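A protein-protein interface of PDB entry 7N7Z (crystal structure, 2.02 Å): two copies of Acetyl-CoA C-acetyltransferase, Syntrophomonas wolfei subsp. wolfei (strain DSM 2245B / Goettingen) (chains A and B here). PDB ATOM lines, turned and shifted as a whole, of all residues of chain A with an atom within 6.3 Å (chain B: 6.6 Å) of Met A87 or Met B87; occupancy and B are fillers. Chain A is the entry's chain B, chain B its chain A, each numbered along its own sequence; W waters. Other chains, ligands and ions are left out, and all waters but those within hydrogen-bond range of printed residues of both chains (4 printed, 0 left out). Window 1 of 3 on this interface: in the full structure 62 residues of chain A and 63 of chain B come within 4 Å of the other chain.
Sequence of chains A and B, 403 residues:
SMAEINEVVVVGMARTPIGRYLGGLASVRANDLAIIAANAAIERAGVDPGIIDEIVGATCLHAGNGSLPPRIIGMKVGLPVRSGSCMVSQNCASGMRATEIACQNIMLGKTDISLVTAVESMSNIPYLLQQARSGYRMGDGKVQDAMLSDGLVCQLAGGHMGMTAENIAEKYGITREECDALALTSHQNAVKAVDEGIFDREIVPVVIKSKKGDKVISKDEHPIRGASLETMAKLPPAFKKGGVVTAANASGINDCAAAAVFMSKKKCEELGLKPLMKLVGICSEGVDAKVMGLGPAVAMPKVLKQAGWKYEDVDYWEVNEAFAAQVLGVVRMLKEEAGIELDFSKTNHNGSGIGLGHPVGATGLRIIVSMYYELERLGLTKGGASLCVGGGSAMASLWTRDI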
ATOM      1  N   ILE A  55     -21.962  23.476 -10.928  1.00  0.00           N
ATOM      2  CA  ILE A  55     -22.979  22.917 -10.049  1.00  0.00           C
ATOM      3  C   ILE A  55     -22.645  21.447  -9.839  1.00  0.00           C
ATOM      4  O   ILE A  55     -22.393  20.720 -10.807  1.00  0.00           O
ATOM      5  CB  ILE A  55     -24.402  23.073 -10.618  1.00  0.00           C
ATOM      6  CG1 ILE A  55     -25.425  22.498  -9.633  1.00  0.00           C
ATOM      7  CG2 ILE A  55     -24.522  22.391 -11.973  1.00  0.00           C
ATOM      8  CD1 ILE A  55     -26.864  22.666 -10.066  1.00  0.00           C
ATOM      9  N   VAL A  56     -22.614  21.022  -8.582  1.00  0.00           N
ATOM     10  CA  VAL A  56     -22.489  19.616  -8.221  1.00  0.00           C
ATOM     11  C   VAL A  56     -23.838  19.190  -7.659  1.00  0.00           C
ATOM     12  O   VAL A  56     -24.208  19.578  -6.543  1.00  0.00           O
ATOM     13  CB  VAL A  56     -21.357  19.378  -7.213  1.00  0.00           C
ATOM     14  CG1 VAL A  56     -21.148  17.888  -6.998  1.00  0.00           C
ATOM     15  CG2 VAL A  56     -20.072  20.035  -7.696  1.00  0.00           C
ATOM     16  N   GLY A  57     -24.583  18.410  -8.438  1.00  0.00           N
ATOM     17  CA  GLY A  57     -25.937  18.027  -8.083  1.00  0.00           C
ATOM     18  C   GLY A  57     -25.970  16.652  -7.441  1.00  0.00           C
ATOM     19  O   GLY A  57     -25.392  15.696  -7.961  1.00  0.00           O
ATOM     20  N   ALA A  58     -26.661  16.568  -6.310  1.00  0.00           N
ATOM     21  CA  ALA A  58     -26.825  15.322  -5.578  1.00  0.00           C
ATOM     22  C   ALA A  58     -28.253  14.818  -5.721  1.00  0.00           C
ATOM     23  O   ALA A  58     -29.209  15.596  -5.645  1.00  0.00           O
ATOM     24  CB  ALA A  58     -26.485  15.506  -4.098  1.00  0.00           C
ATOM     25  N   THR A  59     -28.388  13.512  -5.939  1.00  0.00           N
ATOM     26  CA  THR A  59     -29.682  12.848  -5.989  1.00  0.00           C
ATOM     27  C   THR A  59     -29.437  11.349  -6.025  1.00  0.00           C
ATOM     28  O   THR A  59     -28.418  10.891  -6.551  1.00  0.00           O
ATOM     29  CB  THR A  59     -30.508  13.279  -7.209  1.00  0.00           C
ATOM     30  OG1 THR A  59     -31.884  12.937  -6.998  1.00  0.00           O
ATOM     31  CG2 THR A  59     -30.011  12.592  -8.473  1.00  0.00           C
ATOM     32  N   CYS A  60     -30.377  10.590  -5.463  1.00  0.00           N
ATOM     33  CA  CYS A  60     -30.227   9.141  -5.428  1.00  0.00           C
ATOM     34  C   CYS A  60     -30.893   8.467  -6.624  1.00  0.00           C
ATOM     35  O   CYS A  60     -30.345   7.499  -7.162  1.00  0.00           O
ATOM     36  CB  CYS A  60     -30.793   8.586  -4.115  1.00  0.00           C
ATOM     37  SG  CYS A  60     -30.826   6.774  -4.000  1.00  0.00           S
ATOM     38  N   HIS A  62     -31.940   9.221 -10.263  1.00  0.00           N
ATOM     39  CA  HIS A  62     -31.906  10.037 -11.475  1.00  0.00           C
ATOM     40  C   HIS A  62     -33.138   9.813 -12.345  1.00  0.00           C
ATOM     41  O   HIS A  62     -33.709  10.769 -12.887  1.00  0.00           O
ATOM     42  CB  HIS A  62     -30.628   9.688 -12.245  1.00  0.00           C
ATOM     43  CG  HIS A  62     -30.584  10.189 -13.656  1.00  0.00           C
ATOM     44  ND1 HIS A  62     -29.768   9.616 -14.608  1.00  0.00           N
ATOM     45  CD2 HIS A  62     -31.205  11.224 -14.269  1.00  0.00           C
ATOM     46  CE1 HIS A  62     -29.907  10.261 -15.753  1.00  0.00           C
ATOM     47  NE2 HIS A  62     -30.775  11.240 -15.574  1.00  0.00           N
ATOM     48  N   LEU A  68     -28.798  14.879 -17.520  1.00  0.00           N
ATOM     49  CA  LEU A  68     -27.989  15.581 -16.526  1.00  0.00           C
ATOM     50  C   LEU A  68     -28.795  16.693 -15.863  1.00  0.00           C
ATOM     51  O   LEU A  68     -28.600  17.875 -16.175  1.00  0.00           O
ATOM     52  CB  LEU A  68     -26.721  16.148 -17.168  1.00  0.00           C
ATOM     53  CG  LEU A  68     -25.582  16.530 -16.217  1.00  0.00           C
ATOM     54  CD1 LEU A  68     -25.193  15.359 -15.323  1.00  0.00           C
ATOM     55  CD2 LEU A  68     -24.374  17.024 -17.006  1.00  0.00           C
ATOM     56  N   PRO A  69     -29.705  16.354 -14.955  1.00  0.00           N
ATOM     57  CA  PRO A  69     -30.591  17.365 -14.362  1.00  0.00           C
ATOM     58  C   PRO A  69     -29.820  18.532 -13.768  1.00  0.00           C
ATOM     59  O   PRO A  69     -30.253  19.687 -13.901  1.00  0.00           O
ATOM     60  CB  PRO A  69     -31.342  16.580 -13.277  1.00  0.00           C
ATOM     61  CG  PRO A  69     -31.348  15.170 -13.777  1.00  0.00           C
ATOM     62  CD  PRO A  69     -30.046  14.988 -14.518  1.00  0.00           C
ATOM     63  N   PRO A  70     -28.693  18.290 -13.090  1.00  0.00           N
ATOM     64  CA  PRO A  70     -27.951  19.428 -12.517  1.00  0.00           C
ATOM     65  C   PRO A  70     -27.568  20.480 -13.544  1.00  0.00           C
ATOM     66  O   PRO A  70     -27.534  21.672 -13.212  1.00  0.00           O
ATOM     67  CB  PRO A  70     -26.716  18.764 -11.891  1.00  0.00           C
ATOM     68  CG  PRO A  70     -27.154  17.370 -11.596  1.00  0.00           C
ATOM     69  CD  PRO A  70     -28.072  17.001 -12.727  1.00  0.00           C
ATOM     70  N   SER A  85     -20.698  20.919 -14.552  1.00  0.00           N
ATOM     71  CA  SER A  85     -21.907  20.243 -14.104  1.00  0.00           C
ATOM     72  C   SER A  85     -21.612  18.761 -13.942  1.00  0.00           C
ATOM     73  O   SER A  85     -20.877  18.178 -14.744  1.00  0.00           O
ATOM     74  CB  SER A  85     -23.059  20.449 -15.092  1.00  0.00           C
ATOM     75  OG  SER A  85     -22.802  19.785 -16.318  1.00  0.00           O
ATOM     76  N   CYS A  86     -22.186  18.164 -12.904  1.00  0.00           N
ATOM     77  CA  CYS A  86     -22.083  16.728 -12.695  1.00  0.00           C
ATOM     78  C   CYS A  86     -23.121  16.318 -11.663  1.00  0.00           C
ATOM     79  O   CYS A  86     -23.628  17.147 -10.902  1.00  0.00           O
ATOM     80  CB  CYS A  86     -20.678  16.316 -12.244  1.00  0.00           C
ATOM     81  SG  CYS A  86     -20.351  16.576 -10.488  1.00  0.00           S
ATOM     82  N   MET A  87     -23.433  15.025 -11.655  1.00  0.00           N
ATOM     83  CA  MET A  87     -24.409  14.444 -10.746  1.00  0.00           C
ATOM     84  C   MET A  87     -23.735  13.338  -9.951  1.00  0.00           C
ATOM     85  O   MET A  87     -23.105  12.448 -10.532  1.00  0.00           O
ATOM     86  CB  MET A  87     -25.611  13.893 -11.513  1.00  0.00           C
ATOM     87  CG  MET A  87     -26.709  13.343 -10.628  1.00  0.00           C
ATOM     88  SD  MET A  87     -28.233  13.099 -11.551  1.00  0.00           S
ATOM     89  CE  MET A  87     -27.782  11.660 -12.506  1.00  0.00           C
ATOM     90  N   VAL A  88     -23.868  13.395  -8.629  1.00  0.00           N
ATOM     91  CA  VAL A  88     -23.194  12.471  -7.728  1.00  0.00           C
ATOM     92  C   VAL A  88     -24.242  11.754  -6.893  1.00  0.00           C
ATOM     93  O   VAL A  88     -25.308  12.300  -6.591  1.00  0.00           O
ATOM     94  CB  VAL A  88     -22.175  13.200  -6.823  1.00  0.00           C
ATOM     95  CG1 VAL A  88     -22.829  14.391  -6.145  1.00  0.00           C
ATOM     96  CG2 VAL A  88     -21.579  12.250  -5.784  1.00  0.00           C
ATOM     97  N   SER A  89     -23.928  10.516  -6.518  1.00  0.00           N
ATOM     98  CA  SER A  89     -24.803   9.724  -5.667  1.00  0.00           C
ATOM     99  C   SER A  89     -23.968   8.923  -4.683  1.00  0.00           C
ATOM    100  O   SER A  89     -23.044   8.208  -5.082  1.00  0.00           O
ATOM    101  CB  SER A  89     -25.683   8.782  -6.497  1.00  0.00           C
ATOM    102  OG  SER A  89     -26.546   8.036  -5.656  1.00  0.00           O
ATOM    103  N   GLN A  90     -24.288   9.064  -3.400  1.00  0.00           N
ATOM    104  CA  GLN A  90     -23.803   8.196  -2.331  1.00  0.00           C
ATOM    105  C   GLN A  90     -24.970   7.826  -1.424  1.00  0.00           C
ATOM    106  O   GLN A  90     -24.899   7.907  -0.196  1.00  0.00           O
ATOM    107  CB  GLN A  90     -22.671   8.860  -1.549  1.00  0.00           C
ATOM    108  CG  GLN A  90     -21.872   7.893  -0.677  1.00  0.00           C
ATOM    109  CD  GLN A  90     -20.525   8.452  -0.242  1.00  0.00           C
ATOM    110  OE1 GLN A  90     -19.856   9.155  -0.999  1.00  0.00           O
ATOM    111  NE2 GLN A  90     -20.118   8.130   0.982  1.00  0.00           N
ATOM    112  N   ILE B  55     -14.139   3.351  -4.216  1.00  0.00           N
ATOM    113  CA  ILE B  55     -14.474   3.171  -5.622  1.00  0.00           C
ATOM    114  C   ILE B  55     -15.320   4.361  -6.057  1.00  0.00           C
ATOM    115  O   ILE B  55     -16.297   4.711  -5.388  1.00  0.00           O
ATOM    116  CB  ILE B  55     -15.225   1.852  -5.888  1.00  0.00           C
ATOM    117  CG1 ILE B  55     -15.593   1.757  -7.372  1.00  0.00           C
ATOM    118  CG2 ILE B  55     -16.475   1.752  -5.027  1.00  0.00           C
ATOM    119  CD1 ILE B  55     -15.947   0.360  -7.835  1.00  0.00           C
ATOM    120  N   VAL B  56     -14.938   4.983  -7.167  1.00  0.00           N
ATOM    121  CA  VAL B  56     -15.691   6.079  -7.762  1.00  0.00           C
ATOM    122  C   VAL B  56     -16.221   5.565  -9.094  1.00  0.00           C
ATOM    123  O   VAL B  56     -15.477   5.467 -10.076  1.00  0.00           O
ATOM    124  CB  VAL B  56     -14.833   7.337  -7.939  1.00  0.00           C
ATOM    125  CG1 VAL B  56     -15.679   8.485  -8.466  1.00  0.00           C
ATOM    126  CG2 VAL B  56     -14.174   7.720  -6.621  1.00  0.00           C
ATOM    127  N   GLY B  57     -17.509   5.232  -9.134  1.00  0.00           N
ATOM    128  CA  GLY B  57     -18.105   4.589 -10.290  1.00  0.00           C
ATOM    129  C   GLY B  57     -18.847   5.588 -11.162  1.00  0.00           C
ATOM    130  O   GLY B  57     -19.677   6.358 -10.676  1.00  0.00           O
ATOM    131  N   ALA B  58     -18.540   5.556 -12.453  1.00  0.00           N
ATOM    132  CA  ALA B  58     -19.166   6.431 -13.432  1.00  0.00           C
ATOM    133  C   ALA B  58     -20.137   5.641 -14.298  1.00  0.00           C
ATOM    134  O   ALA B  58     -19.863   4.497 -14.676  1.00  0.00           O
ATOM    135  CB  ALA B  58     -18.114   7.107 -14.317  1.00  0.00           C
ATOM    136  N   THR B  59     -21.274   6.260 -14.599  1.00  0.00           N
ATOM    137  CA  THR B  59     -22.258   5.720 -15.526  1.00  0.00           C
ATOM    138  C   THR B  59     -23.295   6.804 -15.778  1.00  0.00           C
ATOM    139  O   THR B  59     -23.517   7.670 -14.926  1.00  0.00           O
ATOM    140  CB  THR B  59     -22.927   4.449 -14.983  1.00  0.00           C
ATOM    141  OG1 THR B  59     -23.823   3.918 -15.968  1.00  0.00           O
ATOM    142  CG2 THR B  59     -23.704   4.744 -13.704  1.00  0.00           C
ATOM    143  N   CYS B  60     -23.915   6.757 -16.956  1.00  0.00           N
ATOM    144  CA  CYS B  60     -24.913   7.760 -17.306  1.00  0.00           C
ATOM    145  C   CYS B  60     -26.308   7.381 -16.825  1.00  0.00           C
ATOM    146  O   CYS B  60     -27.024   8.229 -16.281  1.00  0.00           O
ATOM    147  CB  CYS B  60     -24.934   7.983 -18.820  1.00  0.00           C
ATOM    148  SG  CYS B  60     -25.983   9.358 -19.341  1.00  0.00           S
ATOM    149  N   LEU B  61     -26.711   6.124 -17.010  1.00  0.00           N
ATOM    150  CA  LEU B  61     -28.039   5.650 -16.625  1.00  0.00           C
ATOM    151  C   LEU B  61     -27.888   4.644 -15.489  1.00  0.00           C
ATOM    152  O   LEU B  61     -27.571   3.472 -15.718  1.00  0.00           O
ATOM    153  CB  LEU B  61     -28.770   5.032 -17.815  1.00  0.00           C
ATOM    154  CG  LEU B  61     -29.342   5.972 -18.885  1.00  0.00           C
ATOM    155  CD1 LEU B  61     -30.244   7.040 -18.277  1.00  0.00           C
ATOM    156  CD2 LEU B  61     -28.225   6.612 -19.703  1.00  0.00           C
ATOM    157  N   HIS B  62     -28.117   5.109 -14.260  1.00  0.00           N
ATOM    158  CA  HIS B  62     -28.130   4.211 -13.111  1.00  0.00           C
ATOM    159  C   HIS B  62     -29.347   3.295 -13.138  1.00  0.00           C
ATOM    160  O   HIS B  62     -29.275   2.156 -12.665  1.00  0.00           O
ATOM    161  CB  HIS B  62     -28.094   5.040 -11.822  1.00  0.00           C
ATOM    162  CG  HIS B  62     -28.617   4.327 -10.611  1.00  0.00           C
ATOM    163  ND1 HIS B  62     -29.447   4.937  -9.695  1.00  0.00           N
ATOM    164  CD2 HIS B  62     -28.408   3.070 -10.149  1.00  0.00           C
ATOM    165  CE1 HIS B  62     -29.740   4.082  -8.730  1.00  0.00           C
ATOM    166  NE2 HIS B  62     -29.122   2.942  -8.983  1.00  0.00           N
ATOM    167  N   GLY B  66     -29.560  -1.519  -9.633  1.00  0.00           N
ATOM    168  CA  GLY B  66     -29.520  -1.767  -8.206  1.00  0.00           C
ATOM    169  C   GLY B  66     -29.089  -0.560  -7.398  1.00  0.00           C
ATOM    170  O   GLY B  66     -28.839   0.535  -7.912  1.00  0.00           O
ATOM    171  N   SER B  67     -28.997  -0.781  -6.087  1.00  0.00           N
ATOM    172  CA  SER B  67     -28.672   0.280  -5.141  1.00  0.00           C
ATOM    173  C   SER B  67     -27.175   0.564  -5.170  1.00  0.00           C
ATOM    174  O   SER B  67     -26.366  -0.323  -4.879  1.00  0.00           O
ATOM    175  CB  SER B  67     -29.113  -0.116  -3.733  1.00  0.00           C
ATOM    176  OG  SER B  67     -28.417   0.634  -2.752  1.00  0.00           O
ATOM    177  N   LEU B  68     -26.813   1.809  -5.506  1.00  0.00           N
ATOM    178  CA  LEU B  68     -25.427   2.258  -5.599  1.00  0.00           C
ATOM    179  C   LEU B  68     -24.545   1.159  -6.182  1.00  0.00           C
ATOM    180  O   LEU B  68     -23.816   0.482  -5.445  1.00  0.00           O
ATOM    181  CB  LEU B  68     -24.913   2.698  -4.226  1.00  0.00           C
ATOM    182  CG  LEU B  68     -23.835   3.786  -4.240  1.00  0.00           C
ATOM    183  CD1 LEU B  68     -24.386   5.096  -4.791  1.00  0.00           C
ATOM    184  CD2 LEU B  68     -23.254   3.997  -2.848  1.00  0.00           C
ATOM    185  N   PRO B  69     -24.584   0.958  -7.497  1.00  0.00           N
ATOM    186  CA  PRO B  69     -23.828  -0.136  -8.116  1.00  0.00           C
ATOM    187  C   PRO B  69     -22.356  -0.098  -7.743  1.00  0.00           C
ATOM    188  O   PRO B  69     -21.767  -1.150  -7.452  1.00  0.00           O
ATOM    189  CB  PRO B  69     -24.034   0.103  -9.620  1.00  0.00           C
ATOM    190  CG  PRO B  69     -25.331   0.829  -9.704  1.00  0.00           C
ATOM    191  CD  PRO B  69     -25.373   1.712  -8.487  1.00  0.00           C
ATOM    192  N   PRO B  70     -21.715   1.077  -7.746  1.00  0.00           N
ATOM    193  CA  PRO B  70     -20.283   1.105  -7.400  1.00  0.00           C
ATOM    194  C   PRO B  70     -19.971   0.434  -6.076  1.00  0.00           C
ATOM    195  O   PRO B  70     -18.903  -0.173  -5.936  1.00  0.00           O
ATOM    196  CB  PRO B  70     -19.961   2.605  -7.373  1.00  0.00           C
ATOM    197  CG  PRO B  70     -20.951   3.209  -8.303  1.00  0.00           C
ATOM    198  CD  PRO B  70     -22.212   2.422  -8.091  1.00  0.00           C
ATOM    199  N   SER B  85     -17.610   4.700  -1.476  1.00  0.00           N
ATOM    200  CA  SER B  85     -18.265   4.396  -2.739  1.00  0.00           C
ATOM    201  C   SER B  85     -19.149   5.568  -3.128  1.00  0.00           C
ATOM    202  O   SER B  85     -19.743   6.218  -2.265  1.00  0.00           O
ATOM    203  CB  SER B  85     -19.100   3.115  -2.645  1.00  0.00           C
ATOM    204  OG  SER B  85     -20.314   3.349  -1.952  1.00  0.00           O
ATOM    205  N   CYS B  86     -19.225   5.835  -4.429  1.00  0.00           N
ATOM    206  CA  CYS B  86     -20.119   6.864  -4.936  1.00  0.00           C
ATOM    207  C   CYS B  86     -20.272   6.679  -6.437  1.00  0.00           C
ATOM    208  O   CYS B  86     -19.440   6.049  -7.094  1.00  0.00           O
ATOM    209  CB  CYS B  86     -19.610   8.275  -4.610  1.00  0.00           C
ATOM    210  SG  CYS B  86     -18.162   8.811  -5.548  1.00  0.00           S
ATOM    211  N   MET B  87     -21.360   7.231  -6.964  1.00  0.00           N
ATOM    212  CA  MET B  87     -21.672   7.190  -8.384  1.00  0.00           C
ATOM    213  C   MET B  87     -21.681   8.614  -8.916  1.00  0.00           C
ATOM    214  O   MET B  87     -22.279   9.503  -8.301  1.00  0.00           O
ATOM    215  CB  MET B  87     -23.028   6.527  -8.628  1.00  0.00           C
ATOM    216  CG  MET B  87     -23.374   6.330 -10.093  1.00  0.00           C
ATOM    217  SD  MET B  87     -24.284   4.799 -10.374  1.00  0.00           S
ATOM    218  CE  MET B  87     -25.578   4.951  -9.151  1.00  0.00           C
ATOM    219  N   VAL B  88     -21.028   8.828 -10.055  1.00  0.00           N
ATOM    220  CA  VAL B  88     -20.925  10.155 -10.645  1.00  0.00           C
ATOM    221  C   VAL B  88     -21.356  10.093 -12.101  1.00  0.00           C
ATOM    222  O   VAL B  88     -21.138   9.094 -12.795  1.00  0.00           O
ATOM    223  CB  VAL B  88     -19.497  10.733 -10.525  1.00  0.00           C
ATOM    224  CG1 VAL B  88     -18.614  10.233 -11.656  1.00  0.00           C
ATOM    225  CG2 VAL B  88     -19.547  12.253 -10.515  1.00  0.00           C
ATOM    226  N   SER B  89     -21.974  11.178 -12.563  1.00  0.00           N
ATOM    227  CA  SER B  89     -22.440  11.280 -13.939  1.00  0.00           C
ATOM    228  C   SER B  89     -22.154  12.678 -14.457  1.00  0.00           C
ATOM    229  O   SER B  89     -22.627  13.667 -13.886  1.00  0.00           O
ATOM    230  CB  SER B  89     -23.937  10.972 -14.044  1.00  0.00           C
ATOM    231  OG  SER B  89     -24.423  11.278 -15.341  1.00  0.00           O
ATOM    232  N   GLN B  90     -21.363  12.756 -15.523  1.00  0.00           N
ATOM    233  CA  GLN B  90     -21.225  13.951 -16.345  1.00  0.00           C
ATOM    234  C   GLN B  90     -21.536  13.596 -17.796  1.00  0.00           C
ATOM    235  O   GLN B  90     -20.832  13.998 -18.726  1.00  0.00           O
ATOM    236  CB  GLN B  90     -19.833  14.563 -16.202  1.00  0.00           C
ATOM    237  CG  GLN B  90     -19.749  16.018 -16.657  1.00  0.00           C
ATOM    238  CD  GLN B  90     -18.576  16.769 -16.042  1.00  0.00           C
ATOM    239  OE1 GLN B  90     -18.126  16.448 -14.942  1.00  0.00           O
ATOM    240  NE2 GLN B  90     -18.082  17.778 -16.753  1.00  0.00           N
HETATM  241  O   HOH W   1     -31.210   6.741 -14.217  1.00  0.00           O
HETATM  242  O   HOH W   2     -31.551   6.131 -11.440  1.00  0.00           O
HETATM  243  O   HOH W   3     -28.941   3.862  -5.209  1.00  0.00           O
HETATM  244  O   HOH W   4     -29.080   8.124  -9.997  1.00  0.00           O
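The backbone carbonyl oxygen (O) of Cys B60 sits close to a ring nitrogen (ND1) of His A62 (3.5 Å).
The backbone carbonyl oxygen (O) of Ser B85 lies close to the side-chain amide oxygen (OE1) of Gln A90 (3.2 Å).
O of Met B87 is in hydrogen-bond range of N of Ser A89 (2.6 Å).
N of Ser B89 is in hydrogen-bond range of O of Met A87 (2.6 Å).
The side-chain amide oxygen (OE1) of Gln B90 lies close to the backbone carbonyl oxygen (O) of Ser A85 (3.3 Å).
The backbone carbonyl oxygen (O) of Ile B55 sits at hydrogen-bond distance from the backbone NH (N) of Cys B86 (3.3 Å).
The backbone carbonyl oxygen (O) of Cys B86 sits at hydrogen-bond distance from the backbone NH (N) of Gly B57 (2.9 Å).
NE2 of His B62 lies within hydrogen-bond range of O of Gly B66 (2.6 Å).
The backbone NH (N) of Gly A57 is in hydrogen-bond range of the backbone carbonyl oxygen (O) of Cys A86 (2.9 Å).
The backbone carbonyl oxygen (O) of Gly A57 is in hydrogen-bond range of the backbone NH (N) of Val A88, at 2.8 Å.
The backbone NH (N) of Thr A59 sits at hydrogen-bond distance from the backbone carbonyl oxygen (O) of Val A88 (3.4 Å).
Among the printed residues, pairs that only touch across the chains: Cys A60 with His B62 (3.7 Å), Leu A68 with Ser B89 (3.4 Å), Cys A86 with Ser B89 (3.3 Å), Cys A86 with Gln B90 (3.7 Å), Met A87 with Met B87 (3.8 Å), Met A87 with Val B88 (3.2 Å), Val A88 with Met B87 (3.2 Å), Ser A89 with Leu B68 (3.4 Å), Ser A89 with Cys B86 (3.2 Å) and Gln A90 with Cys B86 (3.7 Å).
Of chain B, only Met B87, Val B88 and Ser B89 come within 4 Å of Met A87.
Of chain A, only Met A87, Val A88 and Ser A89 come within 4 Å of Met B87.
Printed residues of chain A within 4 Å of Cys B86: Ser A89 and Gln A90.
Printed residues of chain A within 4 Å of Gln B90: Ser A85 and Cys A86.
Of the printed residues of chain B, Leu A68 touches Ser B89.
Of the printed residues of chain A, Ser B89 touches Leu A68 (3.4 Å), Cys A86 (3.3 Å) and Met A87 (2.6 Å).
Printed residues of chain B within 4 Å of Ser A89: Leu B68 (3.4 Å), Cys B86 (3.2 Å) and Met B87 (2.6 Å).
Pro A70 touches none of the printed residues of chain B.
Ser B67 touches none of the printed residues of chain A.
The nearest residue of chain B that does not touch Met A87 is Gln B90 (4.9 Å).
The nearest residue of chain A that does not touch Met B87 is Gln A90 (5.0 Å).
Hydrophobic or aromatic side chains of chain B that line the printed part of chain A: His B62, Leu B68, Met B87 and Val B88.
Of the 16 printed residues of chain A, 9 touch a printed residue of chain B.
Hydrophobic or aromatic side chains of chain A within 4 Å of the printed part of chain B: His A62, Leu A68, Met A87 and Val A88.
Along chain A the printed residues that touch a printed residue of chain B span positions 60 to 90.
Among the printed residues, 15 pairs touch across the chains.
Cys A60 touches His B62, and with the chains exchanged His A62 touches Cys B60.
Met A87 touches its own counterpart, Met B87.
Met A87 touches Val B88, and with the chains exchanged Val A88 touches Met B87.
Met A87 touches Ser B89, and with the chains exchanged Ser A89 touches Met B87.
Water W3 lies within hydrogen-bond range of N of Leu B68 (3.0 Å) and SG of Cys A60 (3.7 Å).
Water W2 lies within hydrogen-bond range of ND1 of His B62 (3.0 Å) and N of His A62 (3.3 Å).
Water W4 lies within hydrogen-bond range of the backbone NH (N) of His A62, the backbone carbonyl oxygen (O) of Cys A60 and a ring nitrogen (ND1) of His B62.
Water W1 bridges a ring nitrogen (ND1) of His A62 (3.2 Å) and the backbone NH of His B62 (3.5 Å).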
